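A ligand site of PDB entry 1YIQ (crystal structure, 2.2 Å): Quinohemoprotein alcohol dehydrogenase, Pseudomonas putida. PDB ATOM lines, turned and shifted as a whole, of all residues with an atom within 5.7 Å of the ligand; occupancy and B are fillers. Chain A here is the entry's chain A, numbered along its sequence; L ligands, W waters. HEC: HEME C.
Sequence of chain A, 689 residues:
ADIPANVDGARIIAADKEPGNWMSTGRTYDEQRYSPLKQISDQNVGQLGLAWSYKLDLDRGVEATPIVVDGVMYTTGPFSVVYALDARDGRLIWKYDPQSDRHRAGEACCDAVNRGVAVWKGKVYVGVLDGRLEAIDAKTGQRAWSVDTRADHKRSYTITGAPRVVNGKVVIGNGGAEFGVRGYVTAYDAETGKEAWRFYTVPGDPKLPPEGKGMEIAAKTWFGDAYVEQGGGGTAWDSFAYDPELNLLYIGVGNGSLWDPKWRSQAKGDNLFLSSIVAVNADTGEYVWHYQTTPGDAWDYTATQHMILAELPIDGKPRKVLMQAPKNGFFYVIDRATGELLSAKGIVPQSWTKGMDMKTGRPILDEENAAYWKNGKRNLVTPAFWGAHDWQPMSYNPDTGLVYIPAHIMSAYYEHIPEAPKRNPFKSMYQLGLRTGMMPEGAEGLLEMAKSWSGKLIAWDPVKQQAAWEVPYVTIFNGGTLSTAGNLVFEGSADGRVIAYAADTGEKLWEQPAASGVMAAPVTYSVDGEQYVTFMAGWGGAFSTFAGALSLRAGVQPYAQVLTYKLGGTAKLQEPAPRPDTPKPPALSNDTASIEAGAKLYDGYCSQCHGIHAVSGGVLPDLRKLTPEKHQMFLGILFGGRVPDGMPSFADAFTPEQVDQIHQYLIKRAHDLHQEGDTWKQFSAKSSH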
ATOM      1  N   ARG A  60       2.477 -15.645  16.222  1.00  0.00           N
ATOM      2  CA  ARG A  60       2.961 -16.923  16.735  1.00  0.00           C
ATOM      3  C   ARG A  60       2.455 -17.007  18.177  1.00  0.00           C
ATOM      4  O   ARG A  60       1.732 -16.107  18.618  1.00  0.00           O
ATOM      5  CB  ARG A  60       4.504 -16.984  16.660  1.00  0.00           C
ATOM      6  CG  ARG A  60       5.025 -16.954  15.209  1.00  0.00           C
ATOM      7  CD  ARG A  60       6.550 -17.035  15.090  1.00  0.00           C
ATOM      8  NE  ARG A  60       7.076 -18.279  15.601  1.00  0.00           N
ATOM      9  CZ  ARG A  60       8.308 -18.738  15.383  1.00  0.00           C
ATOM     10  NH1 ARG A  60       9.157 -18.037  14.643  1.00  0.00           N
ATOM     11  NH2 ARG A  60       8.696 -19.883  15.922  1.00  0.00           N
ATOM     12  N   ALA A 105      17.304 -19.228  16.958  1.00  0.00           N
ATOM     13  CA  ALA A 105      15.870 -19.402  17.077  1.00  0.00           C
ATOM     14  C   ALA A 105      15.468 -20.874  17.159  1.00  0.00           C
ATOM     15  O   ALA A 105      14.471 -21.225  17.799  1.00  0.00           O
ATOM     16  CB  ALA A 105      15.164 -18.730  15.921  1.00  0.00           C
ATOM     17  N   GLY A 106      16.244 -21.738  16.502  1.00  0.00           N
ATOM     18  CA  GLY A 106      15.941 -23.156  16.519  1.00  0.00           C
ATOM     19  C   GLY A 106      16.318 -23.839  17.819  1.00  0.00           C
ATOM     20  O   GLY A 106      16.139 -25.050  17.954  1.00  0.00           O
ATOM     21  N   GLU A 107      16.850 -23.076  18.762  1.00  0.00           N
ATOM     22  CA  GLU A 107      17.237 -23.653  20.043  1.00  0.00           C
ATOM     23  C   GLU A 107      16.029 -23.673  20.972  1.00  0.00           C
ATOM     24  O   GLU A 107      16.101 -24.183  22.090  1.00  0.00           O
ATOM     25  CB  GLU A 107      18.368 -22.846  20.690  1.00  0.00           C
ATOM     26  CG  GLU A 107      19.574 -22.666  19.768  1.00  0.00           C
ATOM     27  CD  GLU A 107      20.776 -22.070  20.453  1.00  0.00           C
ATOM     28  OE1 GLU A 107      20.629 -21.568  21.594  1.00  0.00           O
ATOM     29  OE2 GLU A 107      21.870 -22.112  19.857  1.00  0.00           O
ATOM     30  N   ALA A 108      14.927 -23.113  20.484  1.00  0.00           N
ATOM     31  CA  ALA A 108      13.686 -23.081  21.243  1.00  0.00           C
ATOM     32  C   ALA A 108      12.851 -24.283  20.815  1.00  0.00           C
ATOM     33  O   ALA A 108      12.498 -24.423  19.635  1.00  0.00           O
ATOM     34  CB  ALA A 108      12.942 -21.775  20.984  1.00  0.00           C
ATOM     35  N   SER A 428      19.973 -27.199  16.958  1.00  0.00           N
ATOM     36  CA  SER A 428      18.550 -26.961  16.718  1.00  0.00           C
ATOM     37  C   SER A 428      17.693 -28.193  16.488  1.00  0.00           C
ATOM     38  O   SER A 428      16.627 -28.106  15.874  1.00  0.00           O
ATOM     39  CB  SER A 428      18.380 -25.994  15.538  1.00  0.00           C
ATOM     40  OG  SER A 428      18.999 -24.756  15.796  1.00  0.00           O
ATOM     41  N   TYR A 602      13.467 -35.347   8.069  1.00  0.00           N
ATOM     42  CA  TYR A 602      12.424 -34.424   8.482  1.00  0.00           C
ATOM     43  C   TYR A 602      11.960 -34.700   9.915  1.00  0.00           C
ATOM     44  O   TYR A 602      11.781 -33.768  10.699  1.00  0.00           O
ATOM     45  CB  TYR A 602      11.225 -34.521   7.540  1.00  0.00           C
ATOM     46  CG  TYR A 602      10.112 -33.582   7.920  1.00  0.00           C
ATOM     47  CD1 TYR A 602       9.973 -32.346   7.299  1.00  0.00           C
ATOM     48  CD2 TYR A 602       9.243 -33.902   8.971  1.00  0.00           C
ATOM     49  CE1 TYR A 602       9.004 -31.440   7.716  1.00  0.00           C
ATOM     50  CE2 TYR A 602       8.278 -33.004   9.399  1.00  0.00           C
ATOM     51  CZ  TYR A 602       8.163 -31.773   8.774  1.00  0.00           C
ATOM     52  OH  TYR A 602       7.234 -30.882   9.218  1.00  0.00           O
ATOM     53  N   TYR A 605      14.680 -33.369  12.260  1.00  0.00           N
ATOM     54  CA  TYR A 605      15.111 -31.983  12.196  1.00  0.00           C
ATOM     55  C   TYR A 605      14.061 -30.895  11.959  1.00  0.00           C
ATOM     56  O   TYR A 605      14.336 -29.728  12.223  1.00  0.00           O
ATOM     57  CB  TYR A 605      16.192 -31.838  11.116  1.00  0.00           C
ATOM     58  CG  TYR A 605      17.487 -32.560  11.407  1.00  0.00           C
ATOM     59  CD1 TYR A 605      17.624 -33.926  11.135  1.00  0.00           C
ATOM     60  CD2 TYR A 605      18.581 -31.880  11.931  1.00  0.00           C
ATOM     61  CE1 TYR A 605      18.832 -34.593  11.373  1.00  0.00           C
ATOM     62  CE2 TYR A 605      19.801 -32.535  12.173  1.00  0.00           C
ATOM     63  CZ  TYR A 605      19.924 -33.884  11.891  1.00  0.00           C
ATOM     64  OH  TYR A 605      21.114 -34.518  12.132  1.00  0.00           O
ATOM     65  N   CYS A 606      12.874 -31.246  11.472  1.00  0.00           N
ATOM     66  CA  CYS A 606      11.864 -30.236  11.163  1.00  0.00           C
ATOM     67  C   CYS A 606      10.519 -30.334  11.870  1.00  0.00           C
ATOM     68  O   CYS A 606       9.761 -29.369  11.912  1.00  0.00           O
ATOM     69  CB  CYS A 606      11.558 -30.232   9.663  1.00  0.00           C
ATOM     70  SG  CYS A 606      12.939 -30.745   8.600  1.00  0.00           S
ATOM     71  N   SER A 607      10.204 -31.518  12.401  1.00  0.00           N
ATOM     72  CA  SER A 607       8.903 -31.739  13.029  1.00  0.00           C
ATOM     73  C   SER A 607       8.468 -30.799  14.144  1.00  0.00           C
ATOM     74  O   SER A 607       7.294 -30.419  14.181  1.00  0.00           O
ATOM     75  CB  SER A 607       8.789 -33.198  13.509  1.00  0.00           C
ATOM     76  OG  SER A 607       9.789 -33.511  14.446  1.00  0.00           O
ATOM     77  N   GLN A 608       9.373 -30.409  15.032  1.00  0.00           N
ATOM     78  CA  GLN A 608       8.968 -29.528  16.129  1.00  0.00           C
ATOM     79  C   GLN A 608       8.423 -28.182  15.680  1.00  0.00           C
ATOM     80  O   GLN A 608       7.709 -27.532  16.441  1.00  0.00           O
ATOM     81  CB  GLN A 608      10.097 -29.323  17.150  1.00  0.00           C
ATOM     82  CG  GLN A 608      11.261 -28.430  16.715  1.00  0.00           C
ATOM     83  CD  GLN A 608      12.413 -29.212  16.111  1.00  0.00           C
ATOM     84  OE1 GLN A 608      13.530 -28.702  16.007  1.00  0.00           O
ATOM     85  NE2 GLN A 608      12.148 -30.440  15.680  1.00  0.00           N
ATOM     86  N   CYS A 609       8.740 -27.753  14.464  1.00  0.00           N
ATOM     87  CA  CYS A 609       8.257 -26.459  13.979  1.00  0.00           C
ATOM     88  C   CYS A 609       7.291 -26.556  12.805  1.00  0.00           C
ATOM     89  O   CYS A 609       6.300 -25.802  12.743  1.00  0.00           O
ATOM     90  CB  CYS A 609       9.422 -25.535  13.603  1.00  0.00           C
ATOM     91  SG  CYS A 609      10.536 -25.015  14.969  1.00  0.00           S
ATOM     92  N   HIS A 610       7.538 -27.459  11.867  1.00  0.00           N
ATOM     93  CA  HIS A 610       6.648 -27.565  10.719  1.00  0.00           C
ATOM     94  C   HIS A 610       5.596 -28.679  10.837  1.00  0.00           C
ATOM     95  O   HIS A 610       4.770 -28.863   9.947  1.00  0.00           O
ATOM     96  CB  HIS A 610       7.461 -27.693   9.412  1.00  0.00           C
ATOM     97  CG  HIS A 610       8.166 -26.420   9.025  1.00  0.00           C
ATOM     98  ND1 HIS A 610       7.463 -25.302   8.687  1.00  0.00           N
ATOM     99  CD2 HIS A 610       9.509 -26.387   9.034  1.00  0.00           C
ATOM    100  CE1 HIS A 610       8.492 -24.412   8.443  1.00  0.00           C
ATOM    101  NE2 HIS A 610       9.745 -25.056   8.643  1.00  0.00           N
ATOM    102  N   LEU A 620       3.018 -22.069  11.884  1.00  0.00           N
ATOM    103  CA  LEU A 620       4.262 -21.956  11.137  1.00  0.00           C
ATOM    104  C   LEU A 620       3.991 -22.501   9.740  1.00  0.00           C
ATOM    105  O   LEU A 620       3.042 -23.260   9.541  1.00  0.00           O
ATOM    106  CB  LEU A 620       5.375 -22.742  11.833  1.00  0.00           C
ATOM    107  CG  LEU A 620       6.262 -21.931  12.785  1.00  0.00           C
ATOM    108  CD1 LEU A 620       5.533 -20.719  13.334  1.00  0.00           C
ATOM    109  CD2 LEU A 620       6.724 -22.838  13.898  1.00  0.00           C
ATOM    110  N   PRO A 621       4.818 -22.125   8.756  1.00  0.00           N
ATOM    111  CA  PRO A 621       4.619 -22.599   7.382  1.00  0.00           C
ATOM    112  C   PRO A 621       4.369 -24.088   7.205  1.00  0.00           C
ATOM    113  O   PRO A 621       4.959 -24.912   7.895  1.00  0.00           O
ATOM    114  CB  PRO A 621       5.890 -22.148   6.684  1.00  0.00           C
ATOM    115  CG  PRO A 621       6.219 -20.873   7.408  1.00  0.00           C
ATOM    116  CD  PRO A 621       5.999 -21.258   8.847  1.00  0.00           C
ATOM    117  N   ASP A 622       3.466 -24.429   6.288  1.00  0.00           N
ATOM    118  CA  ASP A 622       3.186 -25.830   5.977  1.00  0.00           C
ATOM    119  C   ASP A 622       4.055 -26.091   4.753  1.00  0.00           C
ATOM    120  O   ASP A 622       3.879 -25.459   3.720  1.00  0.00           O
ATOM    121  CB  ASP A 622       1.712 -26.035   5.639  1.00  0.00           C
ATOM    122  CG  ASP A 622       1.323 -27.500   5.601  1.00  0.00           C
ATOM    123  OD1 ASP A 622       0.502 -27.927   6.454  1.00  0.00           O
ATOM    124  OD2 ASP A 622       1.833 -28.237   4.731  1.00  0.00           O
ATOM    125  N   LEU A 623       4.999 -27.020   4.881  1.00  0.00           N
ATOM    126  CA  LEU A 623       5.915 -27.323   3.801  1.00  0.00           C
ATOM    127  C   LEU A 623       5.309 -28.051   2.603  1.00  0.00           C
ATOM    128  O   LEU A 623       5.989 -28.309   1.614  1.00  0.00           O
ATOM    129  CB  LEU A 623       7.108 -28.120   4.347  1.00  0.00           C
ATOM    130  CG  LEU A 623       7.900 -27.347   5.410  1.00  0.00           C
ATOM    131  CD1 LEU A 623       9.161 -28.095   5.761  1.00  0.00           C
ATOM    132  CD2 LEU A 623       8.222 -25.961   4.885  1.00  0.00           C
ATOM    133  N   LYS A 625       2.609 -26.807   1.111  1.00  0.00           N
ATOM    134  CA  LYS A 625       1.930 -25.754   0.357  1.00  0.00           C
ATOM    135  C   LYS A 625       2.899 -24.701  -0.140  1.00  0.00           C
ATOM    136  O   LYS A 625       2.554 -23.518  -0.228  1.00  0.00           O
ATOM    137  CB  LYS A 625       0.868 -25.090   1.243  1.00  0.00           C
ATOM    138  CG  LYS A 625      -0.043 -26.052   1.994  1.00  0.00           C
ATOM    139  CD  LYS A 625      -0.995 -25.290   2.906  1.00  0.00           C
ATOM    140  CE  LYS A 625      -1.695 -26.205   3.899  1.00  0.00           C
ATOM    141  NZ  LYS A 625      -2.639 -27.135   3.252  1.00  0.00           N
ATOM    142  N   LEU A 626       4.121 -25.118  -0.462  1.00  0.00           N
ATOM    143  CA  LEU A 626       5.143 -24.208  -0.946  1.00  0.00           C
ATOM    144  C   LEU A 626       4.858 -23.733  -2.371  1.00  0.00           C
ATOM    145  O   LEU A 626       4.456 -24.523  -3.221  1.00  0.00           O
ATOM    146  CB  LEU A 626       6.516 -24.900  -0.904  1.00  0.00           C
ATOM    147  CG  LEU A 626       7.105 -25.172   0.469  1.00  0.00           C
ATOM    148  CD1 LEU A 626       8.341 -26.035   0.343  1.00  0.00           C
ATOM    149  CD2 LEU A 626       7.456 -23.867   1.161  1.00  0.00           C
ATOM    150  N   THR A 627       5.060 -22.445  -2.615  1.00  0.00           N
ATOM    151  CA  THR A 627       4.838 -21.902  -3.952  1.00  0.00           C
ATOM    152  C   THR A 627       5.985 -22.367  -4.830  1.00  0.00           C
ATOM    153  O   THR A 627       7.028 -22.796  -4.325  1.00  0.00           O
ATOM    154  CB  THR A 627       4.827 -20.359  -3.961  1.00  0.00           C
ATOM    155  OG1 THR A 627       6.103 -19.877  -3.508  1.00  0.00           O
ATOM    156  CG2 THR A 627       3.718 -19.829  -3.061  1.00  0.00           C
ATOM    157  N   LYS A 630       9.330 -20.842  -3.913  1.00  0.00           N
ATOM    158  CA  LYS A 630       9.987 -21.319  -2.706  1.00  0.00           C
ATOM    159  C   LYS A 630      10.697 -22.632  -2.999  1.00  0.00           C
ATOM    160  O   LYS A 630      11.786 -22.882  -2.484  1.00  0.00           O
ATOM    161  CB  LYS A 630       8.981 -21.501  -1.564  1.00  0.00           C
ATOM    162  CG  LYS A 630       8.334 -20.188  -1.094  1.00  0.00           C
ATOM    163  CD  LYS A 630       9.386 -19.215  -0.561  1.00  0.00           C
ATOM    164  CE  LYS A 630       8.797 -17.850  -0.261  1.00  0.00           C
ATOM    165  NZ  LYS A 630       7.720 -17.897   0.760  1.00  0.00           N
ATOM    166  N   PHE A 634      14.803 -23.730  -2.297  1.00  0.00           N
ATOM    167  CA  PHE A 634      14.722 -24.631  -1.151  1.00  0.00           C
ATOM    168  C   PHE A 634      16.082 -24.866  -0.487  1.00  0.00           C
ATOM    169  O   PHE A 634      16.176 -24.984   0.740  1.00  0.00           O
ATOM    170  CB  PHE A 634      14.103 -25.965  -1.597  1.00  0.00           C
ATOM    171  CG  PHE A 634      13.803 -26.924  -0.469  1.00  0.00           C
ATOM    172  CD1 PHE A 634      14.746 -27.865  -0.082  1.00  0.00           C
ATOM    173  CD2 PHE A 634      12.579 -26.886   0.187  1.00  0.00           C
ATOM    174  CE1 PHE A 634      14.476 -28.763   0.941  1.00  0.00           C
ATOM    175  CE2 PHE A 634      12.298 -27.774   1.212  1.00  0.00           C
ATOM    176  CZ  PHE A 634      13.251 -28.725   1.597  1.00  0.00           C
ATOM    177  N   ILE A 637      17.229 -21.618   1.295  1.00  0.00           N
ATOM    178  CA  ILE A 637      16.437 -21.405   2.498  1.00  0.00           C
ATOM    179  C   ILE A 637      16.923 -22.318   3.607  1.00  0.00           C
ATOM    180  O   ILE A 637      17.180 -21.875   4.723  1.00  0.00           O
ATOM    181  CB  ILE A 637      14.923 -21.669   2.244  1.00  0.00           C
ATOM    182  CG1 ILE A 637      14.370 -20.626   1.266  1.00  0.00           C
ATOM    183  CG2 ILE A 637      14.145 -21.629   3.555  1.00  0.00           C
ATOM    184  CD1 ILE A 637      12.929 -20.850   0.828  1.00  0.00           C
ATOM    185  N   LEU A 638      17.074 -23.595   3.273  1.00  0.00           N
ATOM    186  CA  LEU A 638      17.544 -24.568   4.243  1.00  0.00           C
ATOM    187  C   LEU A 638      18.937 -24.214   4.750  1.00  0.00           C
ATOM    188  O   LEU A 638      19.298 -24.551   5.885  1.00  0.00           O
ATOM    189  CB  LEU A 638      17.548 -25.961   3.619  1.00  0.00           C
ATOM    190  CG  LEU A 638      16.338 -26.834   3.922  1.00  0.00           C
ATOM    191  CD1 LEU A 638      16.369 -27.233   5.395  1.00  0.00           C
ATOM    192  CD2 LEU A 638      15.049 -26.087   3.582  1.00  0.00           C
ATOM    193  N   ARG A 642      16.719 -17.887   5.380  1.00  0.00           N
ATOM    194  CA  ARG A 642      15.547 -17.379   6.069  1.00  0.00           C
ATOM    195  C   ARG A 642      15.752 -17.222   7.571  1.00  0.00           C
ATOM    196  O   ARG A 642      14.776 -17.121   8.326  1.00  0.00           O
ATOM    197  CB  ARG A 642      14.327 -18.273   5.809  1.00  0.00           C
ATOM    198  CG  ARG A 642      13.747 -18.158   4.392  1.00  0.00           C
ATOM    199  CD  ARG A 642      13.136 -16.782   4.120  1.00  0.00           C
ATOM    200  NE  ARG A 642      11.824 -16.601   4.740  1.00  0.00           N
ATOM    201  CZ  ARG A 642      10.729 -17.266   4.393  1.00  0.00           C
ATOM    202  NH1 ARG A 642      10.785 -18.176   3.426  1.00  0.00           N
ATOM    203  NH2 ARG A 642       9.585 -17.044   5.011  1.00  0.00           N
ATOM    204  N   ASP A 645      13.856 -14.795   9.815  1.00  0.00           N
ATOM    205  CA  ASP A 645      12.479 -15.118  10.152  1.00  0.00           C
ATOM    206  C   ASP A 645      12.372 -16.266  11.166  1.00  0.00           C
ATOM    207  O   ASP A 645      11.287 -16.793  11.412  1.00  0.00           O
ATOM    208  CB  ASP A 645      11.689 -15.478   8.890  1.00  0.00           C
ATOM    209  CG  ASP A 645      11.644 -14.345   7.881  1.00  0.00           C
ATOM    210  OD1 ASP A 645      11.395 -13.194   8.292  1.00  0.00           O
ATOM    211  OD2 ASP A 645      11.839 -14.599   6.679  1.00  0.00           O
ATOM    212  N   GLY A 646      13.505 -16.661  11.761  1.00  0.00           N
ATOM    213  CA  GLY A 646      13.477 -17.750  12.731  1.00  0.00           C
ATOM    214  C   GLY A 646      13.641 -19.136  12.130  1.00  0.00           C
ATOM    215  O   GLY A 646      13.554 -20.148  12.830  1.00  0.00           O
ATOM    216  N   MET A 647      13.883 -19.187  10.826  1.00  0.00           N
ATOM    217  CA  MET A 647      14.083 -20.441  10.113  1.00  0.00           C
ATOM    218  C   MET A 647      15.569 -20.737  10.194  1.00  0.00           C
ATOM    219  O   MET A 647      16.361 -20.228   9.393  1.00  0.00           O
ATOM    220  CB  MET A 647      13.629 -20.291   8.660  1.00  0.00           C
ATOM    221  CG  MET A 647      14.024 -21.418   7.711  1.00  0.00           C
ATOM    222  SD  MET A 647      13.645 -23.072   8.304  1.00  0.00           S
ATOM    223  CE  MET A 647      14.913 -23.999   7.484  1.00  0.00           C
ATOM    224  N   PRO A 648      15.983 -21.580  11.152  1.00  0.00           N
ATOM    225  CA  PRO A 648      17.399 -21.914  11.316  1.00  0.00           C
ATOM    226  C   PRO A 648      18.104 -22.414  10.070  1.00  0.00           C
ATOM    227  O   PRO A 648      17.472 -22.878   9.118  1.00  0.00           O
ATOM    228  CB  PRO A 648      17.379 -22.962  12.432  1.00  0.00           C
ATOM    229  CG  PRO A 648      16.051 -23.608  12.276  1.00  0.00           C
ATOM    230  CD  PRO A 648      15.141 -22.438  11.996  1.00  0.00           C
ATOM    231  N   PHE A 650      20.608 -24.978   8.167  1.00  0.00           N
ATOM    232  CA  PHE A 650      20.975 -26.382   8.297  1.00  0.00           C
ATOM    233  C   PHE A 650      22.231 -26.688   7.499  1.00  0.00           C
ATOM    234  O   PHE A 650      22.535 -27.847   7.207  1.00  0.00           O
ATOM    235  CB  PHE A 650      19.813 -27.275   7.867  1.00  0.00           C
ATOM    236  CG  PHE A 650      18.642 -27.208   8.807  1.00  0.00           C
ATOM    237  CD1 PHE A 650      17.770 -26.132   8.783  1.00  0.00           C
ATOM    238  CD2 PHE A 650      18.456 -28.201   9.773  1.00  0.00           C
ATOM    239  CE1 PHE A 650      16.727 -26.031   9.705  1.00  0.00           C
ATOM    240  CE2 PHE A 650      17.419 -28.116  10.699  1.00  0.00           C
ATOM    241  CZ  PHE A 650      16.547 -27.018  10.663  1.00  0.00           C
ATOM    242  N   PHE A 654      23.408 -30.762   7.076  1.00  0.00           N
ATOM    243  CA  PHE A 654      23.019 -31.512   5.883  1.00  0.00           C
ATOM    244  C   PHE A 654      23.934 -31.281   4.694  1.00  0.00           C
ATOM    245  O   PHE A 654      24.581 -30.238   4.587  1.00  0.00           O
ATOM    246  CB  PHE A 654      21.600 -31.129   5.461  1.00  0.00           C
ATOM    247  CG  PHE A 654      20.534 -31.500   6.455  1.00  0.00           C
ATOM    248  CD1 PHE A 654      19.340 -30.781   6.497  1.00  0.00           C
ATOM    249  CD2 PHE A 654      20.692 -32.570   7.326  1.00  0.00           C
ATOM    250  CE1 PHE A 654      18.328 -31.125   7.387  1.00  0.00           C
ATOM    251  CE2 PHE A 654      19.675 -32.920   8.222  1.00  0.00           C
ATOM    252  CZ  PHE A 654      18.501 -32.199   8.249  1.00  0.00           C
ATOM    253  N   ILE A 662      14.895 -34.420   1.566  1.00  0.00           N
ATOM    254  CA  ILE A 662      13.810 -33.863   2.357  1.00  0.00           C
ATOM    255  C   ILE A 662      12.810 -33.245   1.391  1.00  0.00           C
ATOM    256  O   ILE A 662      11.604 -33.451   1.514  1.00  0.00           O
ATOM    257  CB  ILE A 662      14.327 -32.782   3.332  1.00  0.00           C
ATOM    258  CG1 ILE A 662      15.303 -33.408   4.320  1.00  0.00           C
ATOM    259  CG2 ILE A 662      13.157 -32.136   4.057  1.00  0.00           C
ATOM    260  CD1 ILE A 662      15.912 -32.415   5.278  1.00  0.00           C
ATOM    261  N   LEU A 666       8.801 -33.861   0.963  1.00  0.00           N
ATOM    262  CA  LEU A 666       7.792 -32.825   1.094  1.00  0.00           C
ATOM    263  C   LEU A 666       6.886 -32.756  -0.132  1.00  0.00           C
ATOM    264  O   LEU A 666       5.684 -32.526  -0.009  1.00  0.00           O
ATOM    265  CB  LEU A 666       8.464 -31.469   1.343  1.00  0.00           C
ATOM    266  CG  LEU A 666       9.259 -31.392   2.655  1.00  0.00           C
ATOM    267  CD1 LEU A 666       9.898 -30.025   2.786  1.00  0.00           C
ATOM    268  CD2 LEU A 666       8.326 -31.662   3.842  1.00  0.00           C
HETATM  269 FE   HEC L   1      11.579 -24.076   8.475  1.00  0.00          FE
HETATM  270  CHA HEC L   1      10.254 -21.462   6.798  1.00  0.00           C
HETATM  271  CHB HEC L   1      12.017 -25.737   5.540  1.00  0.00           C
HETATM  272  CHC HEC L   1      12.933 -26.741  10.140  1.00  0.00           C
HETATM  273  CHD HEC L   1      11.074 -22.508  11.416  1.00  0.00           C
HETATM  274  NA  HEC L   1      11.202 -23.674   6.521  1.00  0.00           N
HETATM  275  C1A HEC L   1      10.643 -22.530   6.032  1.00  0.00           C
HETATM  276  C2A HEC L   1      10.537 -22.636   4.583  1.00  0.00           C
HETATM  277  C3A HEC L   1      11.029 -23.835   4.232  1.00  0.00           C
HETATM  278  C4A HEC L   1      11.460 -24.498   5.452  1.00  0.00           C
HETATM  279  CMA HEC L   1      11.147 -24.436   2.820  1.00  0.00           C
HETATM  280  CAA HEC L   1       9.945 -21.553   3.660  1.00  0.00           C
HETATM  281  CBA HEC L   1       8.401 -21.662   3.659  1.00  0.00           C
HETATM  282  CGA HEC L   1       7.637 -20.575   2.909  1.00  0.00           C
HETATM  283  O1A HEC L   1       8.225 -19.444   2.826  1.00  0.00           O
HETATM  284  O2A HEC L   1       6.525 -20.847   2.467  1.00  0.00           O
HETATM  285  NB  HEC L   1      12.330 -25.880   7.966  1.00  0.00           N
HETATM  286  C1B HEC L   1      12.417 -26.382   6.666  1.00  0.00           C
HETATM  287  C2B HEC L   1      13.001 -27.704   6.685  1.00  0.00           C
HETATM  288  C3B HEC L   1      13.285 -27.980   7.988  1.00  0.00           C
HETATM  289  C4B HEC L   1      12.858 -26.852   8.767  1.00  0.00           C
HETATM  290  CMB HEC L   1      13.254 -28.570   5.440  1.00  0.00           C
HETATM  291  CAB HEC L   1      13.927 -29.234   8.583  1.00  0.00           C
HETATM  292  CBB HEC L   1      15.409 -29.424   8.172  1.00  0.00           C
HETATM  293  NC  HEC L   1      11.932 -24.518  10.392  1.00  0.00           N
HETATM  294  C1C HEC L   1      12.496 -25.678  10.886  1.00  0.00           C
HETATM  295  C2C HEC L   1      12.564 -25.642  12.336  1.00  0.00           C
HETATM  296  C3C HEC L   1      12.019 -24.473  12.715  1.00  0.00           C
HETATM  297  C4C HEC L   1      11.641 -23.757  11.503  1.00  0.00           C
HETATM  298  CMC HEC L   1      13.116 -26.790  13.220  1.00  0.00           C
HETATM  299  CAC HEC L   1      11.777 -23.938  14.121  1.00  0.00           C
HETATM  300  CBC HEC L   1      13.009 -23.577  14.946  1.00  0.00           C
HETATM  301  ND  HEC L   1      10.829 -22.337   9.001  1.00  0.00           N
HETATM  302  C1D HEC L   1      10.701 -21.826  10.297  1.00  0.00           C
HETATM  303  C2D HEC L   1      10.109 -20.496  10.250  1.00  0.00           C
HETATM  304  C3D HEC L   1       9.878 -20.190   8.920  1.00  0.00           C
HETATM  305  C4D HEC L   1      10.329 -21.352   8.171  1.00  0.00           C
HETATM  306  CMD HEC L   1       9.839 -19.654  11.522  1.00  0.00           C
HETATM  307  CAD HEC L   1       9.259 -18.916   8.238  1.00  0.00           C
HETATM  308  CBD HEC L   1       8.559 -17.871   9.151  1.00  0.00           C
HETATM  309  CGD HEC L   1       8.027 -16.680   8.364  1.00  0.00           C
HETATM  310  O1D HEC L   1       6.960 -16.147   8.698  1.00  0.00           O
HETATM  311  O2D HEC L   1       8.748 -16.307   7.412  1.00  0.00           O
HETATM  312  O   HOH W   1       5.987 -17.781   4.850  1.00  0.00           O
HETATM  313  O   HOH W   2       5.005 -18.120  10.366  1.00  0.00           O
HETATM  314  O   HOH W   3       8.567 -13.469   5.513  1.00  0.00           O
HETATM  315  O   HOH W   4       6.982 -15.487  11.465  1.00  0.00           O
HETATM  316  O   HOH W   5       5.058 -20.556   0.049  1.00  0.00           O
HETATM  317  O   HOH W   6       4.179 -22.559   2.764  1.00  0.00           O
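An iron atom (FE) of the ligand is bound by the side-chain sulfur (SD) of Met 647 (2.3 Å).
NH2 of Arg 642 lies within salt-bridge range of O2D of the ligand (2.6 Å).
An iron atom (FE) of the ligand is bound by a ring nitrogen (NE2) of His 610, 2.1 Å away.
A carbon (CAB) of the ligand is covalently linked to the side-chain sulfur (SG) of Cys 606 (1.8 Å).
The side-chain amino group (NZ) of Lys 630 is in salt-bridge range of an oxygen (O1A) of the ligand (2.6 Å).
The side-chain sulfur (SG) of Cys 609 is covalently linked to a carbon (CAC) of the ligand, 1.8 Å away.
NH1 of Arg 60 touches CMD of the ligand (3.6 Å).
Ala 105 touches the ligand.
Gly 106 touches the ligand.
O of Tyr 605 touches CMC of the ligand, at 3.3 Å.
Gln 608 touches the ligand.
Pro 621 touches the ligand.
Leu 623 touches the ligand.
Leu 626 touches the ligand (CD2 to O2A, 3.4 Å).
Phe 634 touches the ligand.
CG2 of Ile 637 touches C3A of the ligand (3.9 Å).
Leu 638 touches the ligand (CD1 to CMB, 3.4 Å).
Asp 645 touches the ligand.
O of Gly 646 touches CHD of the ligand (3.7 Å).
Pro 648 touches the ligand.
Phe 650 touches the ligand (CE2 to CBB, 3.5 Å).
CE1 of Phe 654 touches CBB of the ligand (3.5 Å).
CG2 of Ile 662 touches CMB of the ligand, at 3.8 Å.
Of the 33 residues printed, 23 come within 4 Å of the ligand.
OH of Tyr 602 lies close to O of His 610 (3.3 Å).
The side-chain carboxylate of Asp 645 lies within salt-bridge range of the guanidinium group of Arg 642, 2.8 Å away.
The backbone carbonyl oxygen (O) of Leu 638 sits at hydrogen-bond distance from the backbone NH (N) of Phe 650.
The backbone NH (N) of Lys 630 sits close to the side-chain hydroxyl (OG1) of Thr 627.
OE1 of Gln 608 sits close to O of Ser 428 (3.2 Å).
The backbone carbonyl oxygen (O) of Pro 621 sits at hydrogen-bond distance from a ring nitrogen (ND1) of His 610 (2.7 Å).
The backbone NH of Met 647 is in hydrogen-bond range of the backbone carbonyl oxygen of Arg 642 (3.4 Å).
Water W5 lies within hydrogen-bond range of an oxygen (O2A) of the ligand and the backbone NH (N) of Thr 627.
Water W6 lies within hydrogen-bond range of O2A of the ligand (2.9 Å) and O of Asp 622 (3.1 Å).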
